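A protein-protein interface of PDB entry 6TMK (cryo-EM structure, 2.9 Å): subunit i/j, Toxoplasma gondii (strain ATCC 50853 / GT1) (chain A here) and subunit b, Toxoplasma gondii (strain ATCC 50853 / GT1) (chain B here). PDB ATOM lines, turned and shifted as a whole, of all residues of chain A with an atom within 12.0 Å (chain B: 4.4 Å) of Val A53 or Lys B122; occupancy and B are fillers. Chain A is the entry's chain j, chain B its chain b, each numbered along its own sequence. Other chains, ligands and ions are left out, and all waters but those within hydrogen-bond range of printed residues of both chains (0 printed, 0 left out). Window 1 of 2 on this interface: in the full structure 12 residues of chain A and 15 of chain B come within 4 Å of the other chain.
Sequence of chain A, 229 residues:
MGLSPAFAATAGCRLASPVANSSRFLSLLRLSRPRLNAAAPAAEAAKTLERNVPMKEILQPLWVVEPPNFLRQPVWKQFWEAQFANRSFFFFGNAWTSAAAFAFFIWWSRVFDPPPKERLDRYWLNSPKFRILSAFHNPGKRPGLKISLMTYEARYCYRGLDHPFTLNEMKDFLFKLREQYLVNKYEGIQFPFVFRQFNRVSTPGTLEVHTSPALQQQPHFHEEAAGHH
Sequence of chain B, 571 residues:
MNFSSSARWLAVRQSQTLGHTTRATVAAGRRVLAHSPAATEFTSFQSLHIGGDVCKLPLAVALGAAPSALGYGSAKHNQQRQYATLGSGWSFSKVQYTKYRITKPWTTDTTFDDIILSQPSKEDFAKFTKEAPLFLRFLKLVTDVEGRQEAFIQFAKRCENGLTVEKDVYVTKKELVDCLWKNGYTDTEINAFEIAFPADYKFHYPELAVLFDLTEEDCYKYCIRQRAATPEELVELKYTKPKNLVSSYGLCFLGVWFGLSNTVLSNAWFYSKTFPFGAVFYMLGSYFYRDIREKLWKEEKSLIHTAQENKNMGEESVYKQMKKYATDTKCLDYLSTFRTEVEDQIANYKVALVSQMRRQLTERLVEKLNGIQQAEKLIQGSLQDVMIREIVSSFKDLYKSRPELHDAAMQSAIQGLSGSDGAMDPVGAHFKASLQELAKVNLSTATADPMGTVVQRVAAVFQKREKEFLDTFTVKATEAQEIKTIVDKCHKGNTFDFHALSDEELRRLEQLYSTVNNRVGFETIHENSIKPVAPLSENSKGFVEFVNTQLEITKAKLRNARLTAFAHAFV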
ATOM      1  N   LYS A  47      -9.580 -29.645  24.699  1.00  0.00           N
ATOM      2  CA  LYS A  47      -9.931 -28.308  25.161  1.00  0.00           C
ATOM      3  C   LYS A  47     -11.435 -28.083  25.060  1.00  0.00           C
ATOM      4  O   LYS A  47     -12.087 -28.577  24.142  1.00  0.00           O
ATOM      5  CB  LYS A  47      -9.184 -27.248  24.351  1.00  0.00           C
ATOM      6  CG  LYS A  47      -9.085 -25.901  25.038  1.00  0.00           C
ATOM      7  CD  LYS A  47      -8.719 -24.805  24.056  1.00  0.00           C
ATOM      8  CE  LYS A  47      -9.942 -24.276  23.329  1.00  0.00           C
ATOM      9  NZ  LYS A  47      -9.588 -23.243  22.318  1.00  0.00           N
ATOM     10  N   THR A  48     -11.977 -27.332  26.012  1.00  0.00           N
ATOM     11  CA  THR A  48     -13.411 -27.114  26.100  1.00  0.00           C
ATOM     12  C   THR A  48     -13.805 -25.843  25.358  1.00  0.00           C
ATOM     13  O   THR A  48     -13.021 -24.898  25.241  1.00  0.00           O
ATOM     14  CB  THR A  48     -13.853 -27.020  27.561  1.00  0.00           C
ATOM     15  OG1 THR A  48     -13.593 -28.265  28.222  1.00  0.00           O
ATOM     16  CG2 THR A  48     -15.334 -26.703  27.663  1.00  0.00           C
ATOM     17  N   LEU A  49     -15.031 -25.838  24.844  1.00  0.00           N
ATOM     18  CA  LEU A  49     -15.588 -24.650  24.216  1.00  0.00           C
ATOM     19  C   LEU A  49     -16.183 -23.733  25.275  1.00  0.00           C
ATOM     20  O   LEU A  49     -17.007 -24.162  26.088  1.00  0.00           O
ATOM     21  CB  LEU A  49     -16.651 -25.046  23.197  1.00  0.00           C
ATOM     22  CG  LEU A  49     -17.307 -23.928  22.393  1.00  0.00           C
ATOM     23  CD1 LEU A  49     -16.283 -23.185  21.579  1.00  0.00           C
ATOM     24  CD2 LEU A  49     -18.363 -24.504  21.490  1.00  0.00           C
ATOM     25  N   GLU A  50     -15.766 -22.467  25.260  1.00  0.00           N
ATOM     26  CA  GLU A  50     -16.332 -21.447  26.126  1.00  0.00           C
ATOM     27  C   GLU A  50     -16.879 -20.246  25.378  1.00  0.00           C
ATOM     28  O   GLU A  50     -17.744 -19.548  25.918  1.00  0.00           O
ATOM     29  CB  GLU A  50     -15.278 -20.954  27.130  1.00  0.00           C
ATOM     30  CG  GLU A  50     -14.035 -20.378  26.479  1.00  0.00           C
ATOM     31  CD  GLU A  50     -12.872 -21.350  26.473  1.00  0.00           C
ATOM     32  OE1 GLU A  50     -11.710 -20.893  26.511  1.00  0.00           O
ATOM     33  OE2 GLU A  50     -13.119 -22.573  26.431  1.00  0.00           O
ATOM     34  N   ARG A  51     -16.409 -19.988  24.163  1.00  0.00           N
ATOM     35  CA  ARG A  51     -16.919 -18.876  23.381  1.00  0.00           C
ATOM     36  C   ARG A  51     -18.404 -19.055  23.106  1.00  0.00           C
ATOM     37  O   ARG A  51     -18.886 -20.173  22.909  1.00  0.00           O
ATOM     38  CB  ARG A  51     -16.147 -18.771  22.070  1.00  0.00           C
ATOM     39  CG  ARG A  51     -16.618 -17.679  21.145  1.00  0.00           C
ATOM     40  CD  ARG A  51     -15.619 -17.462  20.032  1.00  0.00           C
ATOM     41  NE  ARG A  51     -15.899 -18.296  18.870  1.00  0.00           N
ATOM     42  CZ  ARG A  51     -16.835 -18.023  17.967  1.00  0.00           C
ATOM     43  NH1 ARG A  51     -17.588 -16.941  18.093  1.00  0.00           N
ATOM     44  NH2 ARG A  51     -17.022 -18.834  16.938  1.00  0.00           N
ATOM     45  N   ASN A  52     -19.130 -17.941  23.093  1.00  0.00           N
ATOM     46  CA  ASN A  52     -20.542 -17.947  22.738  1.00  0.00           C
ATOM     47  C   ASN A  52     -20.653 -17.870  21.223  1.00  0.00           C
ATOM     48  O   ASN A  52     -20.412 -16.816  20.627  1.00  0.00           O
ATOM     49  CB  ASN A  52     -21.269 -16.786  23.402  1.00  0.00           C
ATOM     50  CG  ASN A  52     -22.763 -16.879  23.248  1.00  0.00           C
ATOM     51  OD1 ASN A  52     -23.279 -17.844  22.693  1.00  0.00           O
ATOM     52  ND2 ASN A  52     -23.471 -15.881  23.746  1.00  0.00           N
ATOM     53  N   VAL A  53     -21.025 -18.981  20.602  1.00  0.00           N
ATOM     54  CA  VAL A  53     -21.047 -19.099  19.149  1.00  0.00           C
ATOM     55  C   VAL A  53     -22.389 -18.568  18.653  1.00  0.00           C
ATOM     56  O   VAL A  53     -23.431 -19.147  18.997  1.00  0.00           O
ATOM     57  CB  VAL A  53     -20.841 -20.551  18.709  1.00  0.00           C
ATOM     58  CG1 VAL A  53     -20.704 -20.638  17.210  1.00  0.00           C
ATOM     59  CG2 VAL A  53     -19.627 -21.126  19.387  1.00  0.00           C
ATOM     60  N   PRO A  54     -22.413 -17.500  17.864  1.00  0.00           N
ATOM     61  CA  PRO A  54     -23.676 -17.064  17.269  1.00  0.00           C
ATOM     62  C   PRO A  54     -24.097 -17.975  16.131  1.00  0.00           C
ATOM     63  O   PRO A  54     -23.310 -18.749  15.585  1.00  0.00           O
ATOM     64  CB  PRO A  54     -23.367 -15.652  16.758  1.00  0.00           C
ATOM     65  CG  PRO A  54     -22.051 -15.292  17.344  1.00  0.00           C
ATOM     66  CD  PRO A  54     -21.328 -16.573  17.525  1.00  0.00           C
ATOM     67  N   MET A  55     -25.371 -17.863  15.775  1.00  0.00           N
ATOM     68  CA  MET A  55     -25.920 -18.681  14.708  1.00  0.00           C
ATOM     69  C   MET A  55     -25.601 -18.132  13.328  1.00  0.00           C
ATOM     70  O   MET A  55     -25.730 -18.864  12.345  1.00  0.00           O
ATOM     71  CB  MET A  55     -27.430 -18.805  14.880  1.00  0.00           C
ATOM     72  CG  MET A  55     -28.092 -19.771  13.932  1.00  0.00           C
ATOM     73  SD  MET A  55     -27.479 -21.445  14.117  1.00  0.00           S
ATOM     74  CE  MET A  55     -28.519 -21.970  15.464  1.00  0.00           C
ATOM     75  N   LYS A  56     -25.208 -16.862  13.222  1.00  0.00           N
ATOM     76  CA  LYS A  56     -24.847 -16.326  11.920  1.00  0.00           C
ATOM     77  C   LYS A  56     -23.523 -16.878  11.421  1.00  0.00           C
ATOM     78  O   LYS A  56     -23.253 -16.814  10.217  1.00  0.00           O
ATOM     79  CB  LYS A  56     -24.792 -14.802  11.973  1.00  0.00           C
ATOM     80  CG  LYS A  56     -23.711 -14.238  12.850  1.00  0.00           C
ATOM     81  CD  LYS A  56     -23.834 -12.734  12.968  1.00  0.00           C
ATOM     82  CE  LYS A  56     -22.898 -12.179  14.025  1.00  0.00           C
ATOM     83  NZ  LYS A  56     -22.827 -10.689  14.008  1.00  0.00           N
ATOM     84  N   GLU A  57     -22.690 -17.411  12.311  1.00  0.00           N
ATOM     85  CA  GLU A  57     -21.477 -18.096  11.896  1.00  0.00           C
ATOM     86  C   GLU A  57     -21.746 -19.483  11.333  1.00  0.00           C
ATOM     87  O   GLU A  57     -20.814 -20.125  10.841  1.00  0.00           O
ATOM     88  CB  GLU A  57     -20.513 -18.209  13.076  1.00  0.00           C
ATOM     89  CG  GLU A  57     -20.080 -16.880  13.648  1.00  0.00           C
ATOM     90  CD  GLU A  57     -18.991 -17.025  14.686  1.00  0.00           C
ATOM     91  OE1 GLU A  57     -18.600 -18.174  14.981  1.00  0.00           O
ATOM     92  OE2 GLU A  57     -18.524 -15.992  15.210  1.00  0.00           O
ATOM     93  N   ILE A  58     -22.986 -19.961  11.395  1.00  0.00           N
ATOM     94  CA  ILE A  58     -23.304 -21.334  11.030  1.00  0.00           C
ATOM     95  C   ILE A  58     -24.330 -21.331   9.909  1.00  0.00           C
ATOM     96  O   ILE A  58     -24.083 -21.859   8.819  1.00  0.00           O
ATOM     97  CB  ILE A  58     -23.824 -22.117  12.243  1.00  0.00           C
ATOM     98  CG1 ILE A  58     -22.746 -22.220  13.310  1.00  0.00           C
ATOM     99  CG2 ILE A  58     -24.230 -23.498  11.831  1.00  0.00           C
ATOM    100  CD1 ILE A  58     -23.281 -22.291  14.689  1.00  0.00           C
ATOM    101  N   LEU A  59     -25.491 -20.746  10.178  1.00  0.00           N
ATOM    102  CA  LEU A  59     -26.591 -20.688   9.230  1.00  0.00           C
ATOM    103  C   LEU A  59     -26.593 -19.314   8.576  1.00  0.00           C
ATOM    104  O   LEU A  59     -26.832 -18.303   9.241  1.00  0.00           O
ATOM    105  CB  LEU A  59     -27.919 -20.953   9.931  1.00  0.00           C
ATOM    106  CG  LEU A  59     -28.072 -22.267  10.686  1.00  0.00           C
ATOM    107  CD1 LEU A  59     -29.416 -22.323  11.361  1.00  0.00           C
ATOM    108  CD2 LEU A  59     -27.910 -23.443   9.760  1.00  0.00           C
ATOM    109  N   GLN A  60     -26.328 -19.281   7.285  1.00  0.00           N
ATOM    110  CA  GLN A  60     -26.356 -18.043   6.526  1.00  0.00           C
ATOM    111  C   GLN A  60     -27.709 -17.890   5.857  1.00  0.00           C
ATOM    112  O   GLN A  60     -28.164 -18.827   5.189  1.00  0.00           O
ATOM    113  CB  GLN A  60     -25.255 -18.032   5.472  1.00  0.00           C
ATOM    114  CG  GLN A  60     -23.874 -18.287   6.020  1.00  0.00           C
ATOM    115  CD  GLN A  60     -23.381 -17.169   6.905  1.00  0.00           C
ATOM    116  OE1 GLN A  60     -23.663 -15.996   6.662  1.00  0.00           O
ATOM    117  NE2 GLN A  60     -22.637 -17.526   7.942  1.00  0.00           N
ATOM    118  N   SER B 121     -28.185 -18.606  20.476  1.00  0.00           N
ATOM    119  CA  SER B 121     -26.766 -18.719  20.757  1.00  0.00           C
ATOM    120  C   SER B 121     -26.511 -19.804  21.801  1.00  0.00           C
ATOM    121  O   SER B 121     -27.431 -20.396  22.379  1.00  0.00           O
ATOM    122  CB  SER B 121     -26.201 -17.377  21.214  1.00  0.00           C
ATOM    123  OG  SER B 121     -26.190 -16.448  20.150  1.00  0.00           O
ATOM    124  N   LYS B 122     -25.224 -20.050  22.041  1.00  0.00           N
ATOM    125  CA  LYS B 122     -24.823 -21.176  22.874  1.00  0.00           C
ATOM    126  C   LYS B 122     -25.319 -21.010  24.301  1.00  0.00           C
ATOM    127  O   LYS B 122     -25.690 -21.991  24.956  1.00  0.00           O
ATOM    128  CB  LYS B 122     -23.308 -21.323  22.838  1.00  0.00           C
ATOM    129  CG  LYS B 122     -22.828 -22.705  23.161  1.00  0.00           C
ATOM    130  CD  LYS B 122     -21.333 -22.737  23.302  1.00  0.00           C
ATOM    131  CE  LYS B 122     -20.905 -23.875  24.185  1.00  0.00           C
ATOM    132  NZ  LYS B 122     -21.017 -23.504  25.613  1.00  0.00           N
ATOM    133  N   GLU B 123     -25.328 -19.777  24.807  1.00  0.00           N
ATOM    134  CA  GLU B 123     -25.824 -19.523  26.150  1.00  0.00           C
ATOM    135  C   GLU B 123     -27.341 -19.446  26.190  1.00  0.00           C
ATOM    136  O   GLU B 123     -27.931 -19.640  27.257  1.00  0.00           O
ATOM    137  CB  GLU B 123     -25.229 -18.231  26.703  1.00  0.00           C
ATOM    138  CG  GLU B 123     -23.755 -18.056  26.418  1.00  0.00           C
ATOM    139  CD  GLU B 123     -22.953 -19.312  26.699  1.00  0.00           C
ATOM    140  OE1 GLU B 123     -22.321 -19.843  25.762  1.00  0.00           O
ATOM    141  OE2 GLU B 123     -22.957 -19.769  27.860  1.00  0.00           O
ATOM    142  N   ASP B 124     -27.981 -19.162  25.056  1.00  0.00           N
ATOM    143  CA  ASP B 124     -29.432 -19.231  24.996  1.00  0.00           C
ATOM    144  C   ASP B 124     -29.904 -20.673  25.045  1.00  0.00           C
ATOM    145  O   ASP B 124     -31.005 -20.951  25.533  1.00  0.00           O
ATOM    146  CB  ASP B 124     -29.943 -18.560  23.725  1.00  0.00           C
ATOM    147  CG  ASP B 124     -29.701 -17.065  23.712  1.00  0.00           C
ATOM    148  OD1 ASP B 124     -29.641 -16.459  24.801  1.00  0.00           O
ATOM    149  OD2 ASP B 124     -29.574 -16.497  22.608  1.00  0.00           O
ATOM    150  N   PHE B 125     -29.091 -21.597  24.544  1.00  0.00           N
ATOM    151  CA  PHE B 125     -29.407 -23.013  24.668  1.00  0.00           C
ATOM    152  C   PHE B 125     -29.422 -23.446  26.129  1.00  0.00           C
ATOM    153  O   PHE B 125     -28.660 -22.947  26.959  1.00  0.00           O
ATOM    154  CB  PHE B 125     -28.393 -23.856  23.899  1.00  0.00           C
ATOM    155  CG  PHE B 125     -28.743 -24.062  22.467  1.00  0.00           C
ATOM    156  CD1 PHE B 125     -29.756 -24.923  22.114  1.00  0.00           C
ATOM    157  CD2 PHE B 125     -28.057 -23.402  21.472  1.00  0.00           C
ATOM    158  CE1 PHE B 125     -30.080 -25.118  20.803  1.00  0.00           C
ATOM    159  CE2 PHE B 125     -28.380 -23.596  20.157  1.00  0.00           C
ATOM    160  CZ  PHE B 125     -29.392 -24.455  19.821  1.00  0.00           C
ATOM    161  N   GLU B 166     -25.158 -28.485  26.560  1.00  0.00           N
ATOM    162  CA  GLU B 166     -26.344 -27.931  25.929  1.00  0.00           C
ATOM    163  C   GLU B 166     -27.241 -29.051  25.424  1.00  0.00           C
ATOM    164  O   GLU B 166     -26.771 -30.050  24.875  1.00  0.00           O
ATOM    165  CB  GLU B 166     -25.944 -27.018  24.775  1.00  0.00           C
ATOM    166  CG  GLU B 166     -25.408 -25.680  25.210  1.00  0.00           C
ATOM    167  CD  GLU B 166     -23.978 -25.755  25.701  1.00  0.00           C
ATOM    168  OE1 GLU B 166     -23.364 -24.690  25.914  1.00  0.00           O
ATOM    169  OE2 GLU B 166     -23.465 -26.880  25.874  1.00  0.00           O
ATOM    170  N   TYR B 205     -21.663 -32.741  21.093  1.00  0.00           N
ATOM    171  CA  TYR B 205     -20.433 -32.258  20.486  1.00  0.00           C
ATOM    172  C   TYR B 205     -19.179 -32.527  21.312  1.00  0.00           C
ATOM    173  O   TYR B 205     -18.134 -32.800  20.698  1.00  0.00           O
ATOM    174  CB  TYR B 205     -20.589 -30.763  20.166  1.00  0.00           C
ATOM    175  CG  TYR B 205     -20.778 -29.850  21.350  1.00  0.00           C
ATOM    176  CD1 TYR B 205     -19.704 -29.187  21.916  1.00  0.00           C
ATOM    177  CD2 TYR B 205     -22.031 -29.635  21.889  1.00  0.00           C
ATOM    178  CE1 TYR B 205     -19.874 -28.352  22.992  1.00  0.00           C
ATOM    179  CE2 TYR B 205     -22.208 -28.803  22.964  1.00  0.00           C
ATOM    180  CZ  TYR B 205     -21.126 -28.163  23.512  1.00  0.00           C
ATOM    181  OH  TYR B 205     -21.296 -27.327  24.590  1.00  0.00           O
ATOM    182  N   TYR B 220     -19.797 -28.631  17.391  1.00  0.00           N
ATOM    183  CA  TYR B 220     -20.989 -27.845  17.672  1.00  0.00           C
ATOM    184  C   TYR B 220     -21.643 -27.381  16.382  1.00  0.00           C
ATOM    185  O   TYR B 220     -22.863 -27.488  16.211  1.00  0.00           O
ATOM    186  CB  TYR B 220     -20.607 -26.658  18.555  1.00  0.00           C
ATOM    187  CG  TYR B 220     -21.719 -25.690  18.867  1.00  0.00           C
ATOM    188  CD1 TYR B 220     -22.572 -25.900  19.933  1.00  0.00           C
ATOM    189  CD2 TYR B 220     -21.902 -24.551  18.106  1.00  0.00           C
ATOM    190  CE1 TYR B 220     -23.580 -25.016  20.220  1.00  0.00           C
ATOM    191  CE2 TYR B 220     -22.905 -23.666  18.387  1.00  0.00           C
ATOM    192  CZ  TYR B 220     -23.741 -23.899  19.442  1.00  0.00           C
ATOM    193  OH  TYR B 220     -24.743 -23.003  19.715  1.00  0.00           O
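The backbone NH (N) of Lys B122 lies within hydrogen-bond range of the side-chain amide oxygen (OD1) of Asn A52, at 3.0 Å.
The side-chain amino group (NZ) of Lys B122 lies within salt-bridge range of the side-chain carboxylate (OE1) of Glu B166 (2.6 Å).
The side-chain carboxylate (OD2) of Asp B124 lies within hydrogen-bond range of the backbone NH (N) of Ser B121 (3.3 Å).
The side-chain amino group of Lys B122 is in salt-bridge range of the side-chain carboxylate of Glu B123.
NH2 of Arg A51 is in salt-bridge range of OE1 of Glu A57 (2.6 Å).
CD2 of Leu A49 touches CE of Lys B122 (3.8 Å).
CD of Lys B122 touches O of Arg A51 (3.6 Å).
Ser B121 touches Asn A52 (CB to OD1, 3.3 Å).
Glu B123 touches Asn A52.
Val A53 touches Ser B121.
Val A53 touches Lys B122.
Val A53 touches Tyr B220 (CB to CE2, 3.8 Å).
Pro A54 touches Ser B121 (CA to OG, 3.9 Å).
CD1 of Ile A58 touches CE2 of Tyr B220 (3.96 Å).
Thr A48 touches none of the printed residues of chain B.
Of the printed residues of chain B, Arg A51 touches Lys B122.
Printed residues of chain B within 4 Å of Asn A52: Ser B121, Lys B122 and Glu B123.
Of chain B, only Ser B121, Lys B122 and Tyr B220 come within 4 Å of Val A53.
Of the printed residues of chain B, Pro A54 touches Ser B121 (3.9 Å).
Ser B121 touches just these residues of chain A: Asn A52, Val A53 and Pro A54.
Lys B122 touches four residues of chain A.
Glu B123 touches just one residue of chain A: Asn A52 (3.5 Å).
No residue of chain A comes within 4 Å of Asp B124.
Tyr B205 touches none of the printed residues of chain A.
Of chain A, only Val A53 and Ile A58 come within 4 Å of Tyr B220.
The nearest residue of chain A that does not touch Lys B122 is Glu A50 (5.1 Å).
Of the 14 printed residues of chain A, 6 touch a printed residue of chain B.
Printed residues of chain B that touch a printed residue of chain A: Ser B121, Lys B122, Glu B123 and Tyr B220.
Among the printed residues, 10 pairs touch across the chains.
Among the printed residues, no Asp or Glu carboxylate lies within 4 Å of a Lys or Arg side-chain nitrogen of the other chain.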
